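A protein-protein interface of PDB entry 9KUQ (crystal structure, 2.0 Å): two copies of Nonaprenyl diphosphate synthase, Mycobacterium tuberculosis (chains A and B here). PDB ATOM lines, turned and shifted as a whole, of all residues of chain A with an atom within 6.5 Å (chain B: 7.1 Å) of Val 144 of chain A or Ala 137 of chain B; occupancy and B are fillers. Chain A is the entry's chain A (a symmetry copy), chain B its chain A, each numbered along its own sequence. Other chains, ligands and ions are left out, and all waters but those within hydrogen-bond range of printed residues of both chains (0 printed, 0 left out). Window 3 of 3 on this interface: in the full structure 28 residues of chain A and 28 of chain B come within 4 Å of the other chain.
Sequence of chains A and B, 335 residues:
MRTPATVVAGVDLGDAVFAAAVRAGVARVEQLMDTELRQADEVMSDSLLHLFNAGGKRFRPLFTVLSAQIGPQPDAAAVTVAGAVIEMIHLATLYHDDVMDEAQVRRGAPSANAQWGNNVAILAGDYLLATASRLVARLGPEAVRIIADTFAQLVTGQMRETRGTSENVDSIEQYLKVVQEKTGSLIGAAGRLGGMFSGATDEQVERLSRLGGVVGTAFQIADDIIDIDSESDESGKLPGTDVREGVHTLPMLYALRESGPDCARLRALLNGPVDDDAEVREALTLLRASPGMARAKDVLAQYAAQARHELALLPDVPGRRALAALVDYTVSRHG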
ATOM      1  N   SER A 133      34.308 -31.047  31.916  1.00  0.00           N
ATOM      2  CA  SER A 133      33.724 -30.885  30.569  1.00  0.00           C
ATOM      3  C   SER A 133      33.043 -32.211  30.165  1.00  0.00           C
ATOM      4  O   SER A 133      31.958 -32.160  29.592  1.00  0.00           O
ATOM      5  CB  SER A 133      34.791 -30.452  29.613  1.00  0.00           C
ATOM      6  OG  SER A 133      34.226 -30.119  28.372  1.00  0.00           O
ATOM      7  N   VAL A 136      29.805 -32.481  32.050  1.00  0.00           N
ATOM      8  CA  VAL A 136      28.744 -31.500  31.664  1.00  0.00           C
ATOM      9  C   VAL A 136      28.193 -31.896  30.285  1.00  0.00           C
ATOM     10  O   VAL A 136      27.032 -31.610  30.025  1.00  0.00           O
ATOM     11  CB  VAL A 136      29.218 -30.038  31.682  1.00  0.00           C
ATOM     12  CG1 VAL A 136      30.206 -29.749  30.553  1.00  0.00           C
ATOM     13  CG2 VAL A 136      28.040 -29.080  31.624  1.00  0.00           C
ATOM     14  N   ALA A 137      28.997 -32.548  29.451  1.00  0.00           N
ATOM     15  CA  ALA A 137      28.555 -33.123  28.159  1.00  0.00           C
ATOM     16  C   ALA A 137      27.346 -34.039  28.407  1.00  0.00           C
ATOM     17  O   ALA A 137      26.450 -34.040  27.588  1.00  0.00           O
ATOM     18  CB  ALA A 137      29.691 -33.862  27.502  1.00  0.00           C
ATOM     19  N   ARG A 138      27.265 -34.721  29.559  1.00  0.00           N
ATOM     20  CA  ARG A 138      26.052 -35.516  29.909  1.00  0.00           C
ATOM     21  C   ARG A 138      24.797 -34.660  30.111  1.00  0.00           C
ATOM     22  O   ARG A 138      23.722 -35.236  29.988  1.00  0.00           O
ATOM     23  CB  ARG A 138      26.236 -36.357  31.179  1.00  0.00           C
ATOM     24  CG  ARG A 138      27.301 -37.423  31.039  1.00  0.00           C
ATOM     25  CD  ARG A 138      27.762 -37.921  32.392  1.00  0.00           C
ATOM     26  NE  ARG A 138      29.074 -38.552  32.259  1.00  0.00           N
ATOM     27  CZ  ARG A 138      29.681 -39.210  33.237  1.00  0.00           C
ATOM     28  NH1 ARG A 138      30.898 -39.689  33.058  1.00  0.00           N
ATOM     29  NH2 ARG A 138      29.062 -39.383  34.394  1.00  0.00           N
ATOM     30  N   LEU A 139      24.874 -33.362  30.435  1.00  0.00           N
ATOM     31  CA  LEU A 139      23.667 -32.567  30.802  1.00  0.00           C
ATOM     32  C   LEU A 139      23.008 -31.915  29.589  1.00  0.00           C
ATOM     33  O   LEU A 139      21.934 -31.298  29.768  1.00  0.00           O
ATOM     34  CB  LEU A 139      24.059 -31.498  31.823  1.00  0.00           C
ATOM     35  CG  LEU A 139      24.678 -32.078  33.098  1.00  0.00           C
ATOM     36  CD1 LEU A 139      25.004 -30.994  34.095  1.00  0.00           C
ATOM     37  CD2 LEU A 139      23.756 -33.118  33.692  1.00  0.00           C
ATOM     38  N   GLY A 140      23.624 -31.948  28.422  1.00  0.00           N
ATOM     39  CA  GLY A 140      22.958 -31.393  27.229  1.00  0.00           C
ATOM     40  C   GLY A 140      23.480 -30.013  26.835  1.00  0.00           C
ATOM     41  O   GLY A 140      24.430 -29.481  27.418  1.00  0.00           O
ATOM     42  N   PRO A 141      22.855 -29.383  25.816  1.00  0.00           N
ATOM     43  CA  PRO A 141      23.491 -28.270  25.117  1.00  0.00           C
ATOM     44  C   PRO A 141      23.584 -27.004  25.979  1.00  0.00           C
ATOM     45  O   PRO A 141      24.631 -26.387  26.040  1.00  0.00           O
ATOM     46  CB  PRO A 141      22.584 -28.055  23.898  1.00  0.00           C
ATOM     47  CG  PRO A 141      21.231 -28.572  24.338  1.00  0.00           C
ATOM     48  CD  PRO A 141      21.521 -29.701  25.305  1.00  0.00           C
ATOM     49  N   GLU A 142      22.480 -26.656  26.604  1.00  0.00           N
ATOM     50  CA  GLU A 142      22.329 -25.386  27.322  1.00  0.00           C
ATOM     51  C   GLU A 142      23.257 -25.436  28.544  1.00  0.00           C
ATOM     52  O   GLU A 142      23.717 -24.383  28.906  1.00  0.00           O
ATOM     53  CB  GLU A 142      20.864 -25.178  27.706  1.00  0.00           C
ATOM     54  CG  GLU A 142      20.404 -23.740  27.536  1.00  0.00           C
ATOM     55  CD  GLU A 142      18.994 -23.574  26.995  1.00  0.00           C
ATOM     56  OE1 GLU A 142      18.062 -24.023  27.684  1.00  0.00           O
ATOM     57  OE2 GLU A 142      18.832 -22.996  25.886  1.00  0.00           O
ATOM     58  N   ALA A 143      23.483 -26.614  29.142  1.00  0.00           N
ATOM     59  CA  ALA A 143      24.312 -26.789  30.363  1.00  0.00           C
ATOM     60  C   ALA A 143      25.748 -26.562  29.969  1.00  0.00           C
ATOM     61  O   ALA A 143      26.478 -25.897  30.707  1.00  0.00           O
ATOM     62  CB  ALA A 143      24.173 -28.156  30.968  1.00  0.00           C
ATOM     63  N   VAL A 144      26.141 -27.156  28.845  1.00  0.00           N
ATOM     64  CA  VAL A 144      27.519 -26.991  28.325  1.00  0.00           C
ATOM     65  C   VAL A 144      27.732 -25.487  28.085  1.00  0.00           C
ATOM     66  O   VAL A 144      28.848 -25.010  28.350  1.00  0.00           O
ATOM     67  CB  VAL A 144      27.724 -27.820  27.047  1.00  0.00           C
ATOM     68  CG1 VAL A 144      29.062 -27.508  26.403  1.00  0.00           C
ATOM     69  CG2 VAL A 144      27.600 -29.315  27.288  1.00  0.00           C
ATOM     70  N   ARG A 145      26.703 -24.813  27.572  1.00  0.00           N
ATOM     71  CA  ARG A 145      26.706 -23.366  27.248  1.00  0.00           C
ATOM     72  C   ARG A 145      26.833 -22.599  28.558  1.00  0.00           C
ATOM     73  O   ARG A 145      27.689 -21.719  28.655  1.00  0.00           O
ATOM     74  CB  ARG A 145      25.416 -23.009  26.495  1.00  0.00           C
ATOM     75  CG  ARG A 145      24.968 -21.555  26.601  1.00  0.00           C
ATOM     76  CD  ARG A 145      25.922 -20.565  25.960  1.00  0.00           C
ATOM     77  NE  ARG A 145      25.533 -20.216  24.598  1.00  0.00           N
ATOM     78  CZ  ARG A 145      25.952 -19.144  23.926  1.00  0.00           C
ATOM     79  NH1 ARG A 145      25.517 -18.938  22.694  1.00  0.00           N
ATOM     80  NH2 ARG A 145      26.800 -18.288  24.480  1.00  0.00           N
ATOM     81  N   ILE A 146      26.024 -22.962  29.554  1.00  0.00           N
ATOM     82  CA  ILE A 146      26.012 -22.254  30.873  1.00  0.00           C
ATOM     83  C   ILE A 146      27.425 -22.316  31.444  1.00  0.00           C
ATOM     84  O   ILE A 146      27.998 -21.254  31.808  1.00  0.00           O
ATOM     85  CB  ILE A 146      24.927 -22.826  31.812  1.00  0.00           C
ATOM     86  CG1 ILE A 146      23.521 -22.443  31.330  1.00  0.00           C
ATOM     87  CG2 ILE A 146      25.153 -22.391  33.258  1.00  0.00           C
ATOM     88  CD1 ILE A 146      22.400 -23.329  31.856  1.00  0.00           C
ATOM     89  N   ILE A 147      28.013 -23.498  31.450  1.00  0.00           N
ATOM     90  CA  ILE A 147      29.320 -23.737  32.120  1.00  0.00           C
ATOM     91  C   ILE A 147      30.419 -22.976  31.362  1.00  0.00           C
ATOM     92  O   ILE A 147      31.236 -22.337  32.020  1.00  0.00           O
ATOM     93  CB  ILE A 147      29.610 -25.242  32.245  1.00  0.00           C
ATOM     94  CG1 ILE A 147      28.746 -25.891  33.333  1.00  0.00           C
ATOM     95  CG2 ILE A 147      31.097 -25.486  32.492  1.00  0.00           C
ATOM     96  CD1 ILE A 147      28.827 -25.209  34.716  1.00  0.00           C
ATOM     97  N   ALA A 148      30.433 -23.075  30.027  1.00  0.00           N
ATOM     98  CA  ALA A 148      31.384 -22.375  29.141  1.00  0.00           C
ATOM     99  C   ALA A 148      31.349 -20.879  29.478  1.00  0.00           C
ATOM    100  O   ALA A 148      32.433 -20.308  29.811  1.00  0.00           O
ATOM    101  CB  ALA A 148      31.001 -22.630  27.710  1.00  0.00           C
ATOM    102  N   ASP A 149      30.153 -20.286  29.450  1.00  0.00           N
ATOM    103  CA  ASP A 149      29.941 -18.850  29.759  1.00  0.00           C
ATOM    104  C   ASP A 149      30.469 -18.548  31.164  1.00  0.00           C
ATOM    105  O   ASP A 149      31.038 -17.467  31.373  1.00  0.00           O
ATOM    106  CB  ASP A 149      28.476 -18.456  29.602  1.00  0.00           C
ATOM    107  CG  ASP A 149      28.047 -18.247  28.156  1.00  0.00           C
ATOM    108  OD1 ASP A 149      28.919 -18.013  27.295  1.00  0.00           O
ATOM    109  OD2 ASP A 149      26.843 -18.345  27.894  1.00  0.00           O
ATOM    110  N   VAL B  81      33.675 -23.877  12.686  1.00  0.00           N
ATOM    111  CA  VAL B  81      33.578 -23.936  14.182  1.00  0.00           C
ATOM    112  C   VAL B  81      34.528 -24.999  14.719  1.00  0.00           C
ATOM    113  O   VAL B  81      35.277 -24.677  15.677  1.00  0.00           O
ATOM    114  CB  VAL B  81      32.163 -24.213  14.701  1.00  0.00           C
ATOM    115  CG1 VAL B  81      32.196 -24.425  16.209  1.00  0.00           C
ATOM    116  CG2 VAL B  81      31.177 -23.153  14.276  1.00  0.00           C
ATOM    117  N   VAL B  85      37.729 -24.451  17.164  1.00  0.00           N
ATOM    118  CA  VAL B  85      37.839 -25.229  18.438  1.00  0.00           C
ATOM    119  C   VAL B  85      39.206 -25.913  18.557  1.00  0.00           C
ATOM    120  O   VAL B  85      39.860 -25.793  19.648  1.00  0.00           O
ATOM    121  CB  VAL B  85      36.766 -26.316  18.574  1.00  0.00           C
ATOM    122  CG1 VAL B  85      37.056 -27.116  19.839  1.00  0.00           C
ATOM    123  CG2 VAL B  85      35.363 -25.711  18.606  1.00  0.00           C
ATOM    124  N   ALA B 130      38.037 -21.994  27.727  1.00  0.00           N
ATOM    125  CA  ALA B 130      36.631 -21.623  28.013  1.00  0.00           C
ATOM    126  C   ALA B 130      35.880 -21.374  26.690  1.00  0.00           C
ATOM    127  O   ALA B 130      34.793 -21.950  26.492  1.00  0.00           O
ATOM    128  CB  ALA B 130      36.602 -20.406  28.902  1.00  0.00           C
ATOM    129  N   THR B 131      36.489 -20.535  25.863  1.00  0.00           N
ATOM    130  CA  THR B 131      36.152 -20.077  24.496  1.00  0.00           C
ATOM    131  C   THR B 131      36.000 -21.244  23.518  1.00  0.00           C
ATOM    132  O   THR B 131      34.951 -21.322  22.870  1.00  0.00           O
ATOM    133  CB  THR B 131      37.271 -19.148  24.039  1.00  0.00           C
ATOM    134  OG1 THR B 131      37.435 -18.299  25.175  1.00  0.00           O
ATOM    135  CG2 THR B 131      36.962 -18.384  22.768  1.00  0.00           C
ATOM    136  N   ALA B 132      37.027 -22.081  23.412  1.00  0.00           N
ATOM    137  CA  ALA B 132      36.966 -23.401  22.748  1.00  0.00           C
ATOM    138  C   ALA B 132      35.662 -24.068  23.155  1.00  0.00           C
ATOM    139  O   ALA B 132      34.969 -24.611  22.299  1.00  0.00           O
ATOM    140  CB  ALA B 132      38.123 -24.290  23.167  1.00  0.00           C
ATOM    141  N   SER B 133      35.396 -24.098  24.457  1.00  0.00           N
ATOM    142  CA  SER B 133      34.242 -24.827  25.022  1.00  0.00           C
ATOM    143  C   SER B 133      32.943 -24.146  24.536  1.00  0.00           C
ATOM    144  O   SER B 133      32.002 -24.858  24.199  1.00  0.00           O
ATOM    145  CB  SER B 133      34.365 -24.872  26.513  1.00  0.00           C
ATOM    146  OG  SER B 133      33.379 -25.710  27.058  1.00  0.00           O
ATOM    147  N   ARG B 134      32.925 -22.813  24.550  1.00  0.00           N
ATOM    148  CA  ARG B 134      31.827 -21.927  24.070  1.00  0.00           C
ATOM    149  C   ARG B 134      31.458 -22.301  22.640  1.00  0.00           C
ATOM    150  O   ARG B 134      30.300 -22.478  22.408  1.00  0.00           O
ATOM    151  CB  ARG B 134      32.194 -20.436  24.076  1.00  0.00           C
ATOM    152  CG  ARG B 134      31.937 -19.702  25.390  1.00  0.00           C
ATOM    153  CD  ARG B 134      31.551 -18.225  25.255  1.00  0.00           C
ATOM    154  NE  ARG B 134      32.592 -17.417  24.624  1.00  0.00           N
ATOM    155  CZ  ARG B 134      32.561 -16.934  23.376  1.00  0.00           C
ATOM    156  NH1 ARG B 134      31.527 -17.162  22.577  1.00  0.00           N
ATOM    157  NH2 ARG B 134      33.574 -16.216  22.938  1.00  0.00           N
ATOM    158  N   LEU B 135      32.438 -22.373  21.735  1.00  0.00           N
ATOM    159  CA  LEU B 135      32.227 -22.732  20.323  1.00  0.00           C
ATOM    160  C   LEU B 135      31.775 -24.186  20.224  1.00  0.00           C
ATOM    161  O   LEU B 135      30.817 -24.449  19.477  1.00  0.00           O
ATOM    162  CB  LEU B 135      33.513 -22.449  19.535  1.00  0.00           C
ATOM    163  CG  LEU B 135      33.533 -21.075  18.880  1.00  0.00           C
ATOM    164  CD1 LEU B 135      33.343 -20.001  19.923  1.00  0.00           C
ATOM    165  CD2 LEU B 135      34.820 -20.866  18.083  1.00  0.00           C
ATOM    166  N   VAL B 136      32.394 -25.112  20.948  1.00  0.00           N
ATOM    167  CA  VAL B 136      32.056 -26.549  20.706  1.00  0.00           C
ATOM    168  C   VAL B 136      30.619 -26.800  21.192  1.00  0.00           C
ATOM    169  O   VAL B 136      29.970 -27.676  20.638  1.00  0.00           O
ATOM    170  CB  VAL B 136      33.047 -27.532  21.347  1.00  0.00           C
ATOM    171  CG1 VAL B 136      32.938 -27.535  22.871  1.00  0.00           C
ATOM    172  CG2 VAL B 136      32.862 -28.935  20.792  1.00  0.00           C
ATOM    173  N   ALA B 137      30.146 -26.041  22.174  1.00  0.00           N
ATOM    174  CA  ALA B 137      28.738 -26.069  22.635  1.00  0.00           C
ATOM    175  C   ALA B 137      27.813 -25.848  21.427  1.00  0.00           C
ATOM    176  O   ALA B 137      26.776 -26.478  21.377  1.00  0.00           O
ATOM    177  CB  ALA B 137      28.519 -25.031  23.703  1.00  0.00           C
ATOM    178  N   ARG B 138      28.222 -25.060  20.423  1.00  0.00           N
ATOM    179  CA  ARG B 138      27.425 -24.920  19.170  1.00  0.00           C
ATOM    180  C   ARG B 138      27.328 -26.218  18.359  1.00  0.00           C
ATOM    181  O   ARG B 138      26.387 -26.298  17.576  1.00  0.00           O
ATOM    182  CB  ARG B 138      27.976 -23.839  18.230  1.00  0.00           C
ATOM    183  CG  ARG B 138      27.911 -22.447  18.819  1.00  0.00           C
ATOM    184  CD  ARG B 138      28.837 -21.498  18.089  1.00  0.00           C
ATOM    185  NE  ARG B 138      29.124 -20.344  18.942  1.00  0.00           N
ATOM    186  CZ  ARG B 138      29.788 -19.272  18.535  1.00  0.00           C
ATOM    187  NH1 ARG B 138      30.070 -18.304  19.389  1.00  0.00           N
ATOM    188  NH2 ARG B 138      30.172 -19.176  17.272  1.00  0.00           N
ATOM    189  N   LEU B 139      28.237 -27.193  18.479  1.00  0.00           N
ATOM    190  CA  LEU B 139      28.248 -28.378  17.574  1.00  0.00           C
ATOM    191  C   LEU B 139      27.391 -29.525  18.105  1.00  0.00           C
ATOM    192  O   LEU B 139      27.254 -30.537  17.382  1.00  0.00           O
ATOM    193  CB  LEU B 139      29.690 -28.849  17.377  1.00  0.00           C
ATOM    194  CG  LEU B 139      30.603 -27.769  16.792  1.00  0.00           C
ATOM    195  CD1 LEU B 139      32.002 -28.292  16.569  1.00  0.00           C
ATOM    196  CD2 LEU B 139      30.007 -27.225  15.515  1.00  0.00           C
ATOM    197  N   GLY B 140      26.899 -29.451  19.327  1.00  0.00           N
ATOM    198  CA  GLY B 140      26.003 -30.515  19.819  1.00  0.00           C
ATOM    199  C   GLY B 140      26.696 -31.499  20.759  1.00  0.00           C
ATOM    200  O   GLY B 140      27.863 -31.341  21.128  1.00  0.00           O
ATOM    201  N   PRO B 141      25.980 -32.567  21.175  1.00  0.00           N
ATOM    202  CA  PRO B 141      26.390 -33.339  22.344  1.00  0.00           C
ATOM    203  C   PRO B 141      27.662 -34.160  22.097  1.00  0.00           C
ATOM    204  O   PRO B 141      28.565 -34.140  22.912  1.00  0.00           O
ATOM    205  CB  PRO B 141      25.180 -34.244  22.611  1.00  0.00           C
ATOM    206  CG  PRO B 141      24.509 -34.386  21.262  1.00  0.00           C
ATOM    207  CD  PRO B 141      24.764 -33.080  20.540  1.00  0.00           C
ATOM    208  N   ALA B 143      29.977 -33.828  19.928  1.00  0.00           N
ATOM    209  CA  ALA B 143      31.167 -32.995  19.615  1.00  0.00           C
ATOM    210  C   ALA B 143      31.768 -32.557  20.925  1.00  0.00           C
ATOM    211  O   ALA B 143      32.993 -32.584  21.065  1.00  0.00           O
ATOM    212  CB  ALA B 143      30.827 -31.783  18.795  1.00  0.00           C
ATOM    213  N   VAL B 144      30.908 -32.116  21.840  1.00  0.00           N
ATOM    214  CA  VAL B 144      31.361 -31.684  23.181  1.00  0.00           C
ATOM    215  C   VAL B 144      32.058 -32.890  23.831  1.00  0.00           C
ATOM    216  O   VAL B 144      33.068 -32.675  24.521  1.00  0.00           O
ATOM    217  CB  VAL B 144      30.178 -31.173  24.020  1.00  0.00           C
ATOM    218  CG1 VAL B 144      30.598 -30.912  25.456  1.00  0.00           C
ATOM    219  CG2 VAL B 144      29.533 -29.929  23.432  1.00  0.00           C
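Ala 137 of chain A touches Val 144 of chain B, and with the chains exchanged Val 144 of chain A touches Ala 137 of chain B. Val 144 of chain B touches its own counterpart, Val 144 of chain A. 9 positions are printed for both chains. Of the 6 pairs that touch across the chains among the printed residues, 3 have their exchanged pair printed and touching as well.
Of the 15 printed residues of chain A, 4 touch a printed residue of chain B. Printed residues of chain A that touch a printed residue of chain B: Ala 137, Val 144, Ala 148 and Asp 149. Hydrophobic or aromatic side chains of chain B that line the printed part of chain A: Ala 137 and Val 144. Among the printed residues, no Asp or Glu carboxylate lies within 4 Å of a Lys or Arg side-chain nitrogen of the other chain.
CG1 of Val 144 of chain B touches CB of Ala 137 of chain A, 3.7 Å away. Ala 137 of chain B touches Val 144 of chain A. Val 144 of chain A touches Val 144 of chain B (CG1 to CG1, 3.9 Å). Ser 133 of chain B touches Ala 148 of chain A. Ala 148 of chain A touches Arg 134 of chain B. Asp 149 of chain A touches Arg 134 of chain B.
Val 144 of chain A touches just these residues of chain B: Ala 137 and Val 144. Of chain A, only Val 144 (3.7 Å) comes within 4 Å of Ala 137 of chain B. Printed residues of chain B within 4 Å of Ala 148 of chain A: Ser 133 and Arg 134. Printed residues of chain A within 4 Å of Arg 134 of chain B: Ala 148 and Asp 149. Printed residues of chain A within 4 Å of Ser 133 of chain B: Ala 148. Val 81 of chain B touches none of the printed residues of chain A. Ser 133 of chain A touches none of the printed residues of chain B.
OD2 of Asp 149 of chain A is in salt-bridge range of NH2 of Arg 145 of chain A, 3.4 Å away.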
